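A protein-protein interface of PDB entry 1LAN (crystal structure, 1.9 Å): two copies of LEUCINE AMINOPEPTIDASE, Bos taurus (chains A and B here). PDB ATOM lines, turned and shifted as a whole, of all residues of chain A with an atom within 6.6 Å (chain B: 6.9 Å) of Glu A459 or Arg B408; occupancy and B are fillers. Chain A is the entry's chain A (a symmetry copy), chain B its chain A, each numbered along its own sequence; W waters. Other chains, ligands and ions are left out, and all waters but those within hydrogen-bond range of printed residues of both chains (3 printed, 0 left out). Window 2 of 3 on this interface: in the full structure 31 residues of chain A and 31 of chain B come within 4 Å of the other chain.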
ATOM      1  N   TRP A  82       4.874  -0.397 -20.081  1.00  0.00           N
ATOM      2  CA  TRP A  82       3.644  -0.021 -20.770  1.00  0.00           C
ATOM      3  C   TRP A  82       3.914   0.978 -21.886  1.00  0.00           C
ATOM      4  O   TRP A  82       5.023   1.514 -22.010  1.00  0.00           O
ATOM      5  CB  TRP A  82       2.557   0.508 -19.798  1.00  0.00           C
ATOM      6  CG  TRP A  82       2.848   1.839 -19.094  1.00  0.00           C
ATOM      7  CD1 TRP A  82       3.828   2.752 -19.404  1.00  0.00           C
ATOM      8  CD2 TRP A  82       2.145   2.385 -17.964  1.00  0.00           C
ATOM      9  NE1 TRP A  82       3.773   3.818 -18.539  1.00  0.00           N
ATOM     10  CE2 TRP A  82       2.751   3.621 -17.649  1.00  0.00           C
ATOM     11  CE3 TRP A  82       1.050   1.955 -17.199  1.00  0.00           C
ATOM     12  CZ2 TRP A  82       2.317   4.422 -16.584  1.00  0.00           C
ATOM     13  CZ3 TRP A  82       0.618   2.749 -16.142  1.00  0.00           C
ATOM     14  CH2 TRP A  82       1.251   3.980 -15.853  1.00  0.00           C
ATOM     15  N   GLY A 369      -0.138  -3.583  -4.108  1.00  0.00           N
ATOM     16  CA  GLY A 369      -1.159  -2.544  -4.160  1.00  0.00           C
ATOM     17  C   GLY A 369      -1.910  -2.543  -5.493  1.00  0.00           C
ATOM     18  O   GLY A 369      -2.201  -3.605  -6.054  1.00  0.00           O
ATOM     19  N   SER A 370      -2.225  -1.353  -6.010  1.00  0.00           N
ATOM     20  CA  SER A 370      -2.933  -1.241  -7.279  1.00  0.00           C
ATOM     21  C   SER A 370      -1.975  -1.042  -8.469  1.00  0.00           C
ATOM     22  O   SER A 370      -2.408  -0.688  -9.577  1.00  0.00           O
ATOM     23  CB  SER A 370      -3.960  -0.104  -7.221  1.00  0.00           C
ATOM     24  OG  SER A 370      -3.345   1.110  -6.845  1.00  0.00           O
ATOM     25  N   GLY A 371      -0.682  -1.256  -8.243  1.00  0.00           N
ATOM     26  CA  GLY A 371       0.287  -1.074  -9.311  1.00  0.00           C
ATOM     27  C   GLY A 371       0.157  -2.121 -10.410  1.00  0.00           C
ATOM     28  O   GLY A 371       0.269  -1.800 -11.597  1.00  0.00           O
ATOM     29  N   GLY A 452      -5.519  -6.396  -4.941  1.00  0.00           N
ATOM     30  CA  GLY A 452      -4.924  -5.074  -4.894  1.00  0.00           C
ATOM     31  C   GLY A 452      -5.426  -4.088  -5.945  1.00  0.00           C
ATOM     32  O   GLY A 452      -5.300  -2.883  -5.759  1.00  0.00           O
ATOM     33  N   THR A 455     -10.036  -1.684  -6.308  1.00  0.00           N
ATOM     34  CA  THR A 455     -10.565  -0.328  -6.280  1.00  0.00           C
ATOM     35  C   THR A 455      -9.602   0.696  -6.811  1.00  0.00           C
ATOM     36  O   THR A 455      -8.395   0.439  -6.937  1.00  0.00           O
ATOM     37  CB  THR A 455     -10.931   0.143  -4.829  1.00  0.00           C
ATOM     38  OG1 THR A 455      -9.732   0.365  -4.078  1.00  0.00           O
ATOM     39  CG2 THR A 455     -11.772  -0.873  -4.101  1.00  0.00           C
ATOM     40  N   ASN A 456     -10.145   1.888  -7.039  1.00  0.00           N
ATOM     41  CA  ASN A 456      -9.373   3.022  -7.500  1.00  0.00           C
ATOM     42  C   ASN A 456      -9.802   4.231  -6.685  1.00  0.00           C
ATOM     43  O   ASN A 456     -10.999   4.419  -6.411  1.00  0.00           O
ATOM     44  CB  ASN A 456      -9.605   3.308  -8.996  1.00  0.00           C
ATOM     45  CG  ASN A 456      -8.591   4.309  -9.558  1.00  0.00           C
ATOM     46  OD1 ASN A 456      -8.918   5.451  -9.880  1.00  0.00           O
ATOM     47  ND2 ASN A 456      -7.339   3.887  -9.637  1.00  0.00           N
ATOM     48  N   LYS A 457      -8.808   4.970  -6.204  1.00  0.00           N
ATOM     49  CA  LYS A 457      -9.019   6.211  -5.474  1.00  0.00           C
ATOM     50  C   LYS A 457      -8.627   7.269  -6.496  1.00  0.00           C
ATOM     51  O   LYS A 457      -9.476   7.990  -6.990  1.00  0.00           O
ATOM     52  CB  LYS A 457      -8.123   6.287  -4.248  1.00  0.00           C
ATOM     53  CG  LYS A 457      -8.435   5.233  -3.200  1.00  0.00           C
ATOM     54  CD  LYS A 457      -7.433   5.286  -2.056  1.00  0.00           C
ATOM     55  CE  LYS A 457      -7.184   3.922  -1.463  1.00  0.00           C
ATOM     56  NZ  LYS A 457      -6.628   2.988  -2.490  1.00  0.00           N
ATOM     57  N   ASP A 458      -7.360   7.251  -6.907  1.00  0.00           N
ATOM     58  CA  ASP A 458      -6.835   8.203  -7.884  1.00  0.00           C
ATOM     59  C   ASP A 458      -5.569   7.723  -8.602  1.00  0.00           C
ATOM     60  O   ASP A 458      -4.952   8.484  -9.338  1.00  0.00           O
ATOM     61  CB  ASP A 458      -6.520   9.525  -7.194  1.00  0.00           C
ATOM     62  CG  ASP A 458      -5.272   9.449  -6.312  1.00  0.00           C
ATOM     63  OD1 ASP A 458      -5.010   8.398  -5.665  1.00  0.00           O
ATOM     64  OD2 ASP A 458      -4.537  10.458  -6.275  1.00  0.00           O
ATOM     65  N   GLU A 459      -5.187   6.470  -8.382  1.00  0.00           N
ATOM     66  CA  GLU A 459      -3.970   5.902  -8.971  1.00  0.00           C
ATOM     67  C   GLU A 459      -4.003   5.889 -10.500  1.00  0.00           C
ATOM     68  O   GLU A 459      -3.031   6.274 -11.160  1.00  0.00           O
ATOM     69  CB  GLU A 459      -3.718   4.490  -8.419  1.00  0.00           C
ATOM     70  CG  GLU A 459      -3.655   4.425  -6.883  1.00  0.00           C
ATOM     71  CD  GLU A 459      -4.975   3.974  -6.250  1.00  0.00           C
ATOM     72  OE1 GLU A 459      -5.996   4.676  -6.387  1.00  0.00           O
ATOM     73  OE2 GLU A 459      -4.992   2.900  -5.618  1.00  0.00           O
ATOM     74  N   VAL A 460      -5.125   5.420 -11.054  1.00  0.00           N
ATOM     75  CA  VAL A 460      -5.354   5.374 -12.499  1.00  0.00           C
ATOM     76  C   VAL A 460      -6.150   6.654 -12.752  1.00  0.00           C
ATOM     77  O   VAL A 460      -7.313   6.748 -12.379  1.00  0.00           O
ATOM     78  CB  VAL A 460      -6.195   4.150 -12.910  1.00  0.00           C
ATOM     79  CG1 VAL A 460      -6.378   4.134 -14.426  1.00  0.00           C
ATOM     80  CG2 VAL A 460      -5.535   2.854 -12.427  1.00  0.00           C
ATOM     81  N   PRO A 461      -5.533   7.637 -13.414  1.00  0.00           N
ATOM     82  CA  PRO A 461      -6.174   8.926 -13.715  1.00  0.00           C
ATOM     83  C   PRO A 461      -7.542   8.874 -14.387  1.00  0.00           C
ATOM     84  O   PRO A 461      -8.444   9.615 -14.002  1.00  0.00           O
ATOM     85  CB  PRO A 461      -5.143   9.614 -14.628  1.00  0.00           C
ATOM     86  CG  PRO A 461      -3.841   8.935 -14.299  1.00  0.00           C
ATOM     87  CD  PRO A 461      -4.257   7.505 -14.141  1.00  0.00           C
ATOM     88  N   TYR A 462      -7.701   7.984 -15.361  1.00  0.00           N
ATOM     89  CA  TYR A 462      -8.953   7.852 -16.109  1.00  0.00           C
ATOM     90  C   TYR A 462     -10.087   7.052 -15.477  1.00  0.00           C
ATOM     91  O   TYR A 462     -11.080   6.777 -16.135  1.00  0.00           O
ATOM     92  CB  TYR A 462      -8.667   7.354 -17.537  1.00  0.00           C
ATOM     93  CG  TYR A 462      -7.717   6.165 -17.630  1.00  0.00           C
ATOM     94  CD1 TYR A 462      -6.332   6.350 -17.722  1.00  0.00           C
ATOM     95  CD2 TYR A 462      -8.208   4.860 -17.675  1.00  0.00           C
ATOM     96  CE1 TYR A 462      -5.461   5.259 -17.869  1.00  0.00           C
ATOM     97  CE2 TYR A 462      -7.350   3.772 -17.815  1.00  0.00           C
ATOM     98  CZ  TYR A 462      -5.987   3.977 -17.912  1.00  0.00           C
ATOM     99  OH  TYR A 462      -5.166   2.880 -18.050  1.00  0.00           O
ATOM    100  N   LEU A 463      -9.940   6.629 -14.225  1.00  0.00           N
ATOM    101  CA  LEU A 463     -11.003   5.884 -13.545  1.00  0.00           C
ATOM    102  C   LEU A 463     -11.420   6.722 -12.335  1.00  0.00           C
ATOM    103  O   LEU A 463     -10.563   7.199 -11.596  1.00  0.00           O
ATOM    104  CB  LEU A 463     -10.516   4.500 -13.068  1.00  0.00           C
ATOM    105  CG  LEU A 463     -10.058   3.446 -14.094  1.00  0.00           C
ATOM    106  CD1 LEU A 463      -9.446   2.231 -13.385  1.00  0.00           C
ATOM    107  CD2 LEU A 463     -11.221   3.009 -14.989  1.00  0.00           C
ATOM    108  N   ARG A 470     -10.502  -4.010 -13.069  1.00  0.00           N
ATOM    109  CA  ARG A 470      -9.208  -4.450 -13.578  1.00  0.00           C
ATOM    110  C   ARG A 470      -9.003  -5.961 -13.284  1.00  0.00           C
ATOM    111  O   ARG A 470      -9.369  -6.438 -12.207  1.00  0.00           O
ATOM    112  CB  ARG A 470      -8.109  -3.615 -12.928  1.00  0.00           C
ATOM    113  CG  ARG A 470      -8.184  -2.130 -13.283  1.00  0.00           C
ATOM    114  CD  ARG A 470      -7.218  -1.285 -12.451  1.00  0.00           C
ATOM    115  NE  ARG A 470      -5.821  -1.635 -12.695  1.00  0.00           N
ATOM    116  CZ  ARG A 470      -4.811  -1.302 -11.905  1.00  0.00           C
ATOM    117  NH1 ARG A 470      -5.037  -0.572 -10.826  1.00  0.00           N
ATOM    118  NH2 ARG A 470      -3.574  -1.673 -12.215  1.00  0.00           N
ATOM    119  N   PHE B 403       7.833   1.445 -10.094  1.00  0.00           N
ATOM    120  CA  PHE B 403       6.946   2.255 -10.931  1.00  0.00           C
ATOM    121  C   PHE B 403       6.738   3.640 -10.333  1.00  0.00           C
ATOM    122  O   PHE B 403       6.676   3.777  -9.105  1.00  0.00           O
ATOM    123  CB  PHE B 403       5.556   1.594 -11.015  1.00  0.00           C
ATOM    124  CG  PHE B 403       5.511   0.270 -11.734  1.00  0.00           C
ATOM    125  CD1 PHE B 403       6.514  -0.120 -12.610  1.00  0.00           C
ATOM    126  CD2 PHE B 403       4.392  -0.561 -11.581  1.00  0.00           C
ATOM    127  CE1 PHE B 403       6.403  -1.308 -13.346  1.00  0.00           C
ATOM    128  CE2 PHE B 403       4.269  -1.751 -12.311  1.00  0.00           C
ATOM    129  CZ  PHE B 403       5.278  -2.126 -13.194  1.00  0.00           C
ATOM    130  N   GLU B 404       6.504   4.637 -11.189  1.00  0.00           N
ATOM    131  CA  GLU B 404       6.253   6.004 -10.725  1.00  0.00           C
ATOM    132  C   GLU B 404       4.960   6.016  -9.903  1.00  0.00           C
ATOM    133  O   GLU B 404       4.764   6.876  -9.051  1.00  0.00           O
ATOM    134  CB  GLU B 404       6.130   6.986 -11.900  1.00  0.00           C
ATOM    135  CG  GLU B 404       5.975   8.480 -11.490  1.00  0.00           C
ATOM    136  CD  GLU B 404       4.532   8.907 -11.146  1.00  0.00           C
ATOM    137  OE1 GLU B 404       3.584   8.402 -11.785  1.00  0.00           O
ATOM    138  OE2 GLU B 404       4.346   9.762 -10.240  1.00  0.00           O
ATOM    139  N   HIS B 405       4.075   5.067 -10.172  1.00  0.00           N
ATOM    140  CA  HIS B 405       2.817   4.924  -9.434  1.00  0.00           C
ATOM    141  C   HIS B 405       3.088   4.958  -7.916  1.00  0.00           C
ATOM    142  O   HIS B 405       2.348   5.586  -7.163  1.00  0.00           O
ATOM    143  CB  HIS B 405       2.193   3.590  -9.851  1.00  0.00           C
ATOM    144  CG  HIS B 405       1.084   3.111  -8.972  1.00  0.00           C
ATOM    145  ND1 HIS B 405       1.277   2.750  -7.657  1.00  0.00           N
ATOM    146  CD2 HIS B 405      -0.208   2.820  -9.256  1.00  0.00           C
ATOM    147  CE1 HIS B 405       0.155   2.251  -7.168  1.00  0.00           C
ATOM    148  NE2 HIS B 405      -0.760   2.283  -8.116  1.00  0.00           N
ATOM    149  N   TYR B 406       4.159   4.298  -7.479  1.00  0.00           N
ATOM    150  CA  TYR B 406       4.530   4.248  -6.055  1.00  0.00           C
ATOM    151  C   TYR B 406       5.221   5.530  -5.573  1.00  0.00           C
ATOM    152  O   TYR B 406       5.038   5.951  -4.429  1.00  0.00           O
ATOM    153  CB  TYR B 406       5.420   3.020  -5.767  1.00  0.00           C
ATOM    154  CG  TYR B 406       4.789   1.705  -6.190  1.00  0.00           C
ATOM    155  CD1 TYR B 406       3.632   1.222  -5.568  1.00  0.00           C
ATOM    156  CD2 TYR B 406       5.327   0.959  -7.241  1.00  0.00           C
ATOM    157  CE1 TYR B 406       3.031   0.032  -5.983  1.00  0.00           C
ATOM    158  CE2 TYR B 406       4.729  -0.232  -7.672  1.00  0.00           C
ATOM    159  CZ  TYR B 406       3.586  -0.693  -7.042  1.00  0.00           C
ATOM    160  OH  TYR B 406       2.993  -1.872  -7.480  1.00  0.00           O
ATOM    161  N   THR B 407       5.988   6.163  -6.459  1.00  0.00           N
ATOM    162  CA  THR B 407       6.697   7.405  -6.134  1.00  0.00           C
ATOM    163  C   THR B 407       5.698   8.502  -5.756  1.00  0.00           C
ATOM    164  O   THR B 407       5.935   9.313  -4.861  1.00  0.00           O
ATOM    165  CB  THR B 407       7.494   7.899  -7.348  1.00  0.00           C
ATOM    166  OG1 THR B 407       8.464   6.918  -7.697  1.00  0.00           O
ATOM    167  CG2 THR B 407       8.182   9.247  -7.059  1.00  0.00           C
ATOM    168  N   ARG B 408       4.582   8.509  -6.465  1.00  0.00           N
ATOM    169  CA  ARG B 408       3.526   9.481  -6.253  1.00  0.00           C
ATOM    170  C   ARG B 408       2.997   9.444  -4.822  1.00  0.00           C
ATOM    171  O   ARG B 408       2.669  10.475  -4.228  1.00  0.00           O
ATOM    172  CB  ARG B 408       2.405   9.189  -7.231  1.00  0.00           C
ATOM    173  CG  ARG B 408       1.560  10.383  -7.548  1.00  0.00           C
ATOM    174  CD  ARG B 408       0.507   9.998  -8.551  1.00  0.00           C
ATOM    175  NE  ARG B 408       1.072   9.319  -9.721  1.00  0.00           N
ATOM    176  CZ  ARG B 408       0.365   8.504 -10.504  1.00  0.00           C
ATOM    177  NH1 ARG B 408      -0.918   8.260 -10.236  1.00  0.00           N
ATOM    178  NH2 ARG B 408       0.930   7.925 -11.553  1.00  0.00           N
ATOM    179  N   GLN B 409       2.974   8.252  -4.238  1.00  0.00           N
ATOM    180  CA  GLN B 409       2.483   8.100  -2.878  1.00  0.00           C
ATOM    181  C   GLN B 409       3.430   8.590  -1.779  1.00  0.00           C
ATOM    182  O   GLN B 409       3.000   8.779  -0.642  1.00  0.00           O
ATOM    183  CB  GLN B 409       2.028   6.663  -2.657  1.00  0.00           C
ATOM    184  CG  GLN B 409       0.824   6.333  -3.552  1.00  0.00           C
ATOM    185  CD  GLN B 409       0.387   4.880  -3.493  1.00  0.00           C
ATOM    186  OE1 GLN B 409      -0.050   4.309  -4.496  1.00  0.00           O
ATOM    187  NE2 GLN B 409       0.515   4.267  -2.322  1.00  0.00           N
ATOM    188  N   VAL B 410       4.694   8.834  -2.117  1.00  0.00           N
ATOM    189  CA  VAL B 410       5.669   9.322  -1.143  1.00  0.00           C
ATOM    190  C   VAL B 410       6.033  10.803  -1.358  1.00  0.00           C
ATOM    191  O   VAL B 410       6.439  11.496  -0.431  1.00  0.00           O
ATOM    192  CB  VAL B 410       6.938   8.412  -1.076  1.00  0.00           C
ATOM    193  CG1 VAL B 410       6.533   6.964  -0.795  1.00  0.00           C
ATOM    194  CG2 VAL B 410       7.756   8.498  -2.353  1.00  0.00           C
ATOM    195  N   ILE B 411       5.855  11.314  -2.571  1.00  0.00           N
ATOM    196  CA  ILE B 411       6.161  12.716  -2.799  1.00  0.00           C
ATOM    197  C   ILE B 411       4.943  13.592  -2.496  1.00  0.00           C
ATOM    198  O   ILE B 411       5.061  14.806  -2.401  1.00  0.00           O
ATOM    199  CB  ILE B 411       6.780  13.000  -4.186  1.00  0.00           C
ATOM    200  CG1 ILE B 411       5.826  12.609  -5.311  1.00  0.00           C
ATOM    201  CG2 ILE B 411       8.127  12.283  -4.299  1.00  0.00           C
ATOM    202  CD1 ILE B 411       6.394  12.874  -6.702  1.00  0.00           C
ATOM    203  N   ASP B 412       3.773  12.977  -2.348  1.00  0.00           N
ATOM    204  CA  ASP B 412       2.569  13.711  -1.963  1.00  0.00           C
ATOM    205  C   ASP B 412       2.857  13.882  -0.465  1.00  0.00           C
ATOM    206  O   ASP B 412       2.624  12.960   0.317  1.00  0.00           O
ATOM    207  CB  ASP B 412       1.327  12.841  -2.192  1.00  0.00           C
ATOM    208  CG  ASP B 412       0.037  13.448  -1.610  1.00  0.00           C
ATOM    209  OD1 ASP B 412       0.001  13.819  -0.412  1.00  0.00           O
ATOM    210  OD2 ASP B 412      -0.978  13.507  -2.338  1.00  0.00           O
ATOM    211  N   CYS B 413       3.403  15.030  -0.079  1.00  0.00           N
ATOM    212  CA  CYS B 413       3.789  15.260   1.307  1.00  0.00           C
ATOM    213  C   CYS B 413       3.369  16.635   1.849  1.00  0.00           C
ATOM    214  O   CYS B 413       3.647  17.652   1.238  1.00  0.00           O
ATOM    215  CB  CYS B 413       5.308  15.094   1.383  1.00  0.00           C
ATOM    216  SG  CYS B 413       6.025  15.345   2.976  1.00  0.00           S
ATOM    217  N   LYS B 423       0.966   7.309   1.544  1.00  0.00           N
ATOM    218  CA  LYS B 423      -0.375   7.789   1.858  1.00  0.00           C
ATOM    219  C   LYS B 423      -1.282   6.643   2.270  1.00  0.00           C
ATOM    220  O   LYS B 423      -2.208   6.834   3.065  1.00  0.00           O
ATOM    221  CB  LYS B 423      -1.010   8.457   0.644  1.00  0.00           C
ATOM    222  CG  LYS B 423      -0.411   9.759   0.245  1.00  0.00           C
ATOM    223  CD  LYS B 423      -0.129   9.753  -1.242  1.00  0.00           C
ATOM    224  CE  LYS B 423      -1.389   9.477  -2.070  1.00  0.00           C
ATOM    225  NZ  LYS B 423      -2.380  10.584  -1.986  1.00  0.00           N
ATOM    226  N   TYR B 424      -1.052   5.476   1.666  1.00  0.00           N
ATOM    227  CA  TYR B 424      -1.849   4.272   1.914  1.00  0.00           C
ATOM    228  C   TYR B 424      -0.968   3.167   2.480  1.00  0.00           C
ATOM    229  O   TYR B 424       0.254   3.222   2.397  1.00  0.00           O
ATOM    230  CB  TYR B 424      -2.473   3.772   0.607  1.00  0.00           C
ATOM    231  CG  TYR B 424      -3.086   4.852  -0.266  1.00  0.00           C
ATOM    232  CD1 TYR B 424      -4.057   5.728   0.234  1.00  0.00           C
ATOM    233  CD2 TYR B 424      -2.704   4.989  -1.598  1.00  0.00           C
ATOM    234  CE1 TYR B 424      -4.628   6.712  -0.580  1.00  0.00           C
ATOM    235  CE2 TYR B 424      -3.267   5.964  -2.420  1.00  0.00           C
ATOM    236  CZ  TYR B 424      -4.231   6.825  -1.911  1.00  0.00           C
ATOM    237  OH  TYR B 424      -4.793   7.773  -2.738  1.00  0.00           O
ATOM    238  N   SER B 426      -1.115   0.042   1.392  1.00  0.00           N
ATOM    239  CA  SER B 426      -0.873  -0.934   0.348  1.00  0.00           C
ATOM    240  C   SER B 426       0.546  -0.823  -0.233  1.00  0.00           C
ATOM    241  O   SER B 426       1.121   0.268  -0.273  1.00  0.00           O
ATOM    242  CB  SER B 426      -1.879  -0.721  -0.777  1.00  0.00           C
ATOM    243  OG  SER B 426      -3.207  -0.771  -0.282  1.00  0.00           O
ATOM    244  N   ALA B 434      10.411   3.137  -3.687  1.00  0.00           N
ATOM    245  CA  ALA B 434      10.209   4.396  -4.414  1.00  0.00           C
ATOM    246  C   ALA B 434      10.881   5.524  -3.639  1.00  0.00           C
ATOM    247  O   ALA B 434      11.535   6.385  -4.233  1.00  0.00           O
ATOM    248  CB  ALA B 434       8.722   4.679  -4.595  1.00  0.00           C
HETATM  249  O   HOH W   1      -0.796   0.967  -4.844  1.00  0.00           O
HETATM  250  O   HOH W   2      -4.648   1.533  -1.433  1.00  0.00           O
HETATM  251  O   HOH W   3      -0.677   5.731 -10.194  1.00  0.00           O
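OH of Tyr B424 lies within hydrogen-bond range of OD1 of Asp A458 (3.0 Å).
The side-chain hydroxyl (OG) of Ser A370 is in hydrogen-bond range of a ring nitrogen (NE2) of His B405 (3.1 Å).
The guanidinium group (NH1) of Arg B408 is in hydrogen-bond range of the backbone carbonyl oxygen (O) of Glu A459.
NZ of Lys A457 lies within salt-bridge range of OE2 of Glu A459, 3.5 Å away.
The backbone carbonyl oxygen of Ser A370 sits at hydrogen-bond distance from the guanidinium group of Arg A470, at 2.9 Å.
The side-chain carboxylate (OE2) of Glu A459 sits at hydrogen-bond distance from the side-chain hydroxyl (OG) of Ser A370 (2.7 Å).
The backbone NH (N) of Ser A370 sits close to the backbone carbonyl oxygen (O) of Gly A452 (3.4 Å).
NH2 of Arg B408 is in salt-bridge range of OE1 of Glu B404 (2.7 Å).
Ser B426 touches Gly A369 (CB to CA, 3.9 Å).
Gly A371 touches His B405.
OH of Tyr B406 touches CA of Gly A371 (3.4 Å).
Tyr B424 touches Lys A457.
CB of Glu A459 touches NE2 of His B405, 3.7 Å away.
Glu A459 touches just these residues of chain B: His B405 and Arg B408.
Arg B408 touches just one residue of chain A: Glu A459 (3.0 Å).
Of the printed residues of chain B, Lys A457 touches Tyr B424.
Printed residues of chain B within 4 Å of Ser A370: His B405 (3.1 Å).
The nearest residue of chain B that does not touch Glu A459 is Gln B409 (4.3 Å).
Of the 15 printed residues of chain B, 5 touch a printed residue of chain A.
Printed residues of chain B that touch a printed residue of chain A: His B405, Tyr B406, Arg B408, Tyr B424 and Ser B426.
Among the printed residues, 8 pairs touch across the chains.
Among the printed residues, no Asp or Glu carboxylate lies within 4 Å of a Lys or Arg side-chain nitrogen of the other chain.
No position is printed for both chains.
Of the 8 pairs that touch across the chains among the printed residues, none has its exchanged pair printed and touching as well.
Water W3 lies within hydrogen-bond range of the guanidinium group (NH1) of Arg B408 (2.5 Å) and the backbone carbonyl oxygen (O) of Glu A459 (2.6 Å).
Water W2 lies within hydrogen-bond range of the side-chain amino group of Lys A457 (2.7 Å) and the side-chain hydroxyl of Ser B426 (3.0 Å).
Water W1 bridges N of Ser A370 (3.0 Å) and OE1 of Gln B409 (3.4 Å).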
